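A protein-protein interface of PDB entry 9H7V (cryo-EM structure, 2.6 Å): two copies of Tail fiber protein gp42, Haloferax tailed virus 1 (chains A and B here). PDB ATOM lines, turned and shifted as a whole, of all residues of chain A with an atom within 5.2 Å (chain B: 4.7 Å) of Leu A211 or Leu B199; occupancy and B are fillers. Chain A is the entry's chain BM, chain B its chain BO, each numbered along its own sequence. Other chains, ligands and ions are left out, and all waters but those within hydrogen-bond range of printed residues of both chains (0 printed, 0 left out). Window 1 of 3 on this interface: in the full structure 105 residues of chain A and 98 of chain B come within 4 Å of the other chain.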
ATOM      1  N   VAL A 193     -22.751 -17.211 -16.334  1.00  0.00           N
ATOM      2  CA  VAL A 193     -21.730 -18.098 -16.876  1.00  0.00           C
ATOM      3  C   VAL A 193     -20.785 -17.274 -17.752  1.00  0.00           C
ATOM      4  O   VAL A 193     -21.225 -16.622 -18.699  1.00  0.00           O
ATOM      5  CB  VAL A 193     -22.340 -19.302 -17.629  1.00  0.00           C
ATOM      6  CG1 VAL A 193     -21.291 -20.118 -18.373  1.00  0.00           C
ATOM      7  CG2 VAL A 193     -23.145 -20.206 -16.705  1.00  0.00           C
ATOM      8  N   LEU A 199     -16.115 -21.111 -25.176  1.00  0.00           N
ATOM      9  CA  LEU A 199     -17.353 -21.819 -24.901  1.00  0.00           C
ATOM     10  C   LEU A 199     -17.589 -22.845 -26.010  1.00  0.00           C
ATOM     11  O   LEU A 199     -17.709 -22.487 -27.181  1.00  0.00           O
ATOM     12  CB  LEU A 199     -18.508 -20.814 -24.777  1.00  0.00           C
ATOM     13  CG  LEU A 199     -19.926 -21.386 -24.677  1.00  0.00           C
ATOM     14  CD1 LEU A 199     -20.052 -22.411 -23.556  1.00  0.00           C
ATOM     15  CD2 LEU A 199     -20.933 -20.268 -24.465  1.00  0.00           C
ATOM     16  N   HIS A 207     -16.779 -22.148 -29.952  1.00  0.00           N
ATOM     17  CA  HIS A 207     -16.867 -20.761 -30.380  1.00  0.00           C
ATOM     18  C   HIS A 207     -15.724 -19.966 -29.755  1.00  0.00           C
ATOM     19  O   HIS A 207     -15.661 -19.814 -28.535  1.00  0.00           O
ATOM     20  CB  HIS A 207     -18.243 -20.165 -30.045  1.00  0.00           C
ATOM     21  CG  HIS A 207     -19.376 -20.973 -30.578  1.00  0.00           C
ATOM     22  ND1 HIS A 207     -19.726 -20.961 -31.912  1.00  0.00           N
ATOM     23  CD2 HIS A 207     -20.217 -21.835 -29.970  1.00  0.00           C
ATOM     24  CE1 HIS A 207     -20.742 -21.774 -32.104  1.00  0.00           C
ATOM     25  NE2 HIS A 207     -21.065 -22.318 -30.926  1.00  0.00           N
ATOM     26  N   GLY A 209     -15.249 -16.778 -30.697  1.00  0.00           N
ATOM     27  CA  GLY A 209     -15.739 -15.406 -30.673  1.00  0.00           C
ATOM     28  C   GLY A 209     -17.040 -15.244 -29.885  1.00  0.00           C
ATOM     29  O   GLY A 209     -17.273 -15.963 -28.915  1.00  0.00           O
ATOM     30  N   GLU A 210     -17.869 -14.279 -30.318  1.00  0.00           N
ATOM     31  CA  GLU A 210     -19.137 -13.952 -29.677  1.00  0.00           C
ATOM     32  C   GLU A 210     -20.182 -15.017 -30.007  1.00  0.00           C
ATOM     33  O   GLU A 210     -20.024 -15.776 -30.963  1.00  0.00           O
ATOM     34  CB  GLU A 210     -19.701 -12.612 -30.170  1.00  0.00           C
ATOM     35  CG  GLU A 210     -18.767 -11.417 -30.063  1.00  0.00           C
ATOM     36  CD  GLU A 210     -19.206 -10.167 -30.812  1.00  0.00           C
ATOM     37  OE1 GLU A 210     -20.428  -9.967 -30.985  1.00  0.00           O
ATOM     38  OE2 GLU A 210     -18.320  -9.390 -31.224  1.00  0.00           O
ATOM     39  N   LEU A 211     -21.252 -15.050 -29.198  1.00  0.00           N
ATOM     40  CA  LEU A 211     -22.490 -15.739 -29.535  1.00  0.00           C
ATOM     41  C   LEU A 211     -23.520 -14.715 -30.016  1.00  0.00           C
ATOM     42  O   LEU A 211     -23.326 -13.512 -29.845  1.00  0.00           O
ATOM     43  CB  LEU A 211     -23.005 -16.509 -28.313  1.00  0.00           C
ATOM     44  CG  LEU A 211     -22.322 -17.841 -27.995  1.00  0.00           C
ATOM     45  CD1 LEU A 211     -22.953 -18.466 -26.762  1.00  0.00           C
ATOM     46  CD2 LEU A 211     -22.399 -18.813 -29.167  1.00  0.00           C
ATOM     47  N   GLU A 212     -24.617 -15.213 -30.609  1.00  0.00           N
ATOM     48  CA  GLU A 212     -25.633 -14.384 -31.244  1.00  0.00           C
ATOM     49  C   GLU A 212     -26.983 -14.576 -30.553  1.00  0.00           C
ATOM     50  O   GLU A 212     -27.466 -15.702 -30.438  1.00  0.00           O
ATOM     51  CB  GLU A 212     -25.735 -14.715 -32.737  1.00  0.00           C
ATOM     52  CG  GLU A 212     -24.485 -14.373 -33.538  1.00  0.00           C
ATOM     53  CD  GLU A 212     -24.269 -12.910 -33.897  1.00  0.00           C
ATOM     54  OE1 GLU A 212     -24.762 -12.023 -33.163  1.00  0.00           O
ATOM     55  OE2 GLU A 212     -23.601 -12.655 -34.918  1.00  0.00           O
ATOM     56  N   ASP A 213     -27.582 -13.459 -30.104  1.00  0.00           N
ATOM     57  CA  ASP A 213     -28.922 -13.430 -29.529  1.00  0.00           C
ATOM     58  C   ASP A 213     -29.960 -13.456 -30.651  1.00  0.00           C
ATOM     59  O   ASP A 213     -29.614 -13.277 -31.819  1.00  0.00           O
ATOM     60  CB  ASP A 213     -29.173 -12.169 -28.690  1.00  0.00           C
ATOM     61  CG  ASP A 213     -28.012 -11.706 -27.827  1.00  0.00           C
ATOM     62  OD1 ASP A 213     -26.977 -11.303 -28.399  1.00  0.00           O
ATOM     63  OD2 ASP A 213     -28.163 -11.729 -26.588  1.00  0.00           O
ATOM     64  N   ALA B 195     -27.775 -21.248 -17.404  1.00  0.00           N
ATOM     65  CA  ALA B 195     -27.381 -19.880 -17.112  1.00  0.00           C
ATOM     66  C   ALA B 195     -28.617 -18.996 -16.960  1.00  0.00           C
ATOM     67  O   ALA B 195     -29.089 -18.413 -17.936  1.00  0.00           O
ATOM     68  CB  ALA B 195     -26.455 -19.370 -18.192  1.00  0.00           C
ATOM     69  N   THR B 198     -27.636 -14.244 -16.782  1.00  0.00           N
ATOM     70  CA  THR B 198     -26.547 -13.728 -17.623  1.00  0.00           C
ATOM     71  C   THR B 198     -25.750 -14.859 -18.285  1.00  0.00           C
ATOM     72  O   THR B 198     -25.595 -15.929 -17.699  1.00  0.00           O
ATOM     73  CB  THR B 198     -25.601 -12.810 -16.824  1.00  0.00           C
ATOM     74  OG1 THR B 198     -26.244 -11.551 -16.616  1.00  0.00           O
ATOM     75  CG2 THR B 198     -24.260 -12.550 -17.480  1.00  0.00           C
ATOM     76  N   LEU B 199     -25.239 -14.602 -19.503  1.00  0.00           N
ATOM     77  CA  LEU B 199     -24.169 -15.379 -20.123  1.00  0.00           C
ATOM     78  C   LEU B 199     -23.176 -14.434 -20.802  1.00  0.00           C
ATOM     79  O   LEU B 199     -23.575 -13.583 -21.594  1.00  0.00           O
ATOM     80  CB  LEU B 199     -24.762 -16.392 -21.115  1.00  0.00           C
ATOM     81  CG  LEU B 199     -23.820 -16.961 -22.183  1.00  0.00           C
ATOM     82  CD1 LEU B 199     -22.751 -17.865 -21.579  1.00  0.00           C
ATOM     83  CD2 LEU B 199     -24.603 -17.710 -23.253  1.00  0.00           C
ATOM     84  N   THR B 200     -21.882 -14.610 -20.489  1.00  0.00           N
ATOM     85  CA  THR B 200     -20.791 -13.877 -21.119  1.00  0.00           C
ATOM     86  C   THR B 200     -19.941 -14.850 -21.938  1.00  0.00           C
ATOM     87  O   THR B 200     -19.387 -15.803 -21.392  1.00  0.00           O
ATOM     88  CB  THR B 200     -19.966 -13.097 -20.084  1.00  0.00           C
ATOM     89  OG1 THR B 200     -20.853 -12.261 -19.339  1.00  0.00           O
ATOM     90  CG2 THR B 200     -18.874 -12.248 -20.701  1.00  0.00           C
ATOM     91  N   ASP B 201     -19.831 -14.578 -23.245  1.00  0.00           N
ATOM     92  CA  ASP B 201     -19.227 -15.491 -24.209  1.00  0.00           C
ATOM     93  C   ASP B 201     -17.703 -15.349 -24.219  1.00  0.00           C
ATOM     94  O   ASP B 201     -17.131 -14.660 -23.377  1.00  0.00           O
ATOM     95  CB  ASP B 201     -19.860 -15.329 -25.595  1.00  0.00           C
ATOM     96  CG  ASP B 201     -19.813 -13.914 -26.157  1.00  0.00           C
ATOM     97  OD1 ASP B 201     -18.823 -13.195 -25.900  1.00  0.00           O
ATOM     98  OD2 ASP B 201     -20.767 -13.541 -26.862  1.00  0.00           O
ATOM     99  N   VAL B 205     -19.282 -10.614 -24.704  1.00  0.00           N
ATOM    100  CA  VAL B 205     -20.616 -10.037 -24.820  1.00  0.00           C
ATOM    101  C   VAL B 205     -21.546 -10.729 -23.820  1.00  0.00           C
ATOM    102  O   VAL B 205     -21.615 -11.956 -23.786  1.00  0.00           O
ATOM    103  CB  VAL B 205     -21.154 -10.086 -26.268  1.00  0.00           C
ATOM    104  CG1 VAL B 205     -22.594  -9.599 -26.374  1.00  0.00           C
ATOM    105  CG2 VAL B 205     -20.270  -9.304 -27.231  1.00  0.00           C
ATOM    106  N   SER B 206     -22.269  -9.917 -23.031  1.00  0.00           N
ATOM    107  CA  SER B 206     -23.061 -10.383 -21.898  1.00  0.00           C
ATOM    108  C   SER B 206     -24.552 -10.451 -22.243  1.00  0.00           C
ATOM    109  O   SER B 206     -25.300  -9.500 -22.008  1.00  0.00           O
ATOM    110  CB  SER B 206     -22.795  -9.543 -20.667  1.00  0.00           C
ATOM    111  OG  SER B 206     -21.425  -9.605 -20.295  1.00  0.00           O
ATOM    112  N   HIS B 207     -24.966 -11.610 -22.779  1.00  0.00           N
ATOM    113  CA  HIS B 207     -26.330 -11.928 -23.186  1.00  0.00           C
ATOM    114  C   HIS B 207     -27.237 -12.071 -21.960  1.00  0.00           C
ATOM    115  O   HIS B 207     -26.759 -12.421 -20.881  1.00  0.00           O
ATOM    116  CB  HIS B 207     -26.312 -13.206 -24.042  1.00  0.00           C
ATOM    117  CG  HIS B 207     -25.241 -13.206 -25.081  1.00  0.00           C
ATOM    118  ND1 HIS B 207     -25.397 -12.568 -26.292  1.00  0.00           N
ATOM    119  CD2 HIS B 207     -23.997 -13.732 -25.090  1.00  0.00           C
ATOM    120  CE1 HIS B 207     -24.306 -12.711 -27.012  1.00  0.00           C
ATOM    121  NE2 HIS B 207     -23.432 -13.422 -26.297  1.00  0.00           N
ATOM    122  N   LEU B 211     -31.011 -17.398 -27.721  1.00  0.00           N
ATOM    123  CA  LEU B 211     -29.857 -17.404 -28.611  1.00  0.00           C
ATOM    124  C   LEU B 211     -30.210 -18.028 -29.962  1.00  0.00           C
ATOM    125  O   LEU B 211     -31.201 -18.749 -30.076  1.00  0.00           O
ATOM    126  CB  LEU B 211     -28.723 -18.191 -27.941  1.00  0.00           C
ATOM    127  CG  LEU B 211     -28.287 -17.731 -26.547  1.00  0.00           C
ATOM    128  CD1 LEU B 211     -27.356 -18.751 -25.909  1.00  0.00           C
ATOM    129  CD2 LEU B 211     -27.618 -16.363 -26.594  1.00  0.00           C
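Leu A211 touches just these residues of chain B: Leu B199 (3.95 Å), Asp B201 (2.8 Å) and His B207 (3.1 Å).
Printed residues of chain A within 4 Å of Val B205: Glu A210.
Of the printed residues of chain B, Val A193 touches Ala B195, Thr B198, Leu B199 and Thr B200.
Leu A199 touches none of the printed residues of chain B.
The nearest residue of chain B that does not touch Leu A211 is Leu B211 (4.5 Å).
The nearest residue of chain A that does not touch Leu B199 is Leu A199 (4.2 Å).
The nearest printed residue of chain A that does not touch Thr B198 is Asp A213 (9.2 Å).
The side-chain carboxylate (OD2) of Asp B201 sits at hydrogen-bond distance from the backbone NH (N) of Leu A211, 2.8 Å away.
The backbone carbonyl oxygen (O) of Val A193 lies within hydrogen-bond range of the backbone NH (N) of Thr B200.
The backbone carbonyl oxygen of Thr B198 lies within hydrogen-bond range of the backbone NH of Val A193 (3.4 Å).
A ring nitrogen (ND1) of His B207 is in hydrogen-bond range of the side-chain carboxylate (OD2) of Asp A213, 2.9 Å away.
OD1 of Asp B201 lies within hydrogen-bond range of N of Val B205 (2.9 Å).
O of Val B205 lies close to NE2 of His B207 (3.4 Å).
The side-chain hydroxyl (OG) of Ser B206 sits at hydrogen-bond distance from the side-chain hydroxyl (OG1) of Thr B200 (2.9 Å).
A ring nitrogen (NE2) of His B207 is in hydrogen-bond range of the side-chain carboxylate (OD2) of Asp B201.
The backbone carbonyl oxygen of Leu B199 is in hydrogen-bond range of the backbone NH of His B207 (2.7 Å).
Of the 9 printed residues of chain B, 8 touch a printed residue of chain A.
Along chain B the printed residues that touch a printed residue of chain A span positions 195 to 211.
Of the 8 printed residues of chain A, 5 touch a printed residue of chain B.
Val A193 touches Ala B195 (CG2 to CB, 3.7 Å).
Val A193 touches Leu B199.
Asp B201 touches Glu A210 (OD2 to CA, 3.3 Å).
Val B205 touches Glu A210.
CD2 of Leu B199 touches CD1 of Leu A211, 3.95 Å away.
His B207 touches Leu A211.
O of Glu A212 touches CA of Leu B211, at 3.5 Å.
Leu A211 touches Leu B199, but with the chains exchanged Leu A199 does not touch Leu B211 (6.8 Å).
Leu A211 touches His B207, but with the chains exchanged His A207 does not touch Leu B211 (8.8 Å).
Positions printed for both chains: 199, 207 and 211.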
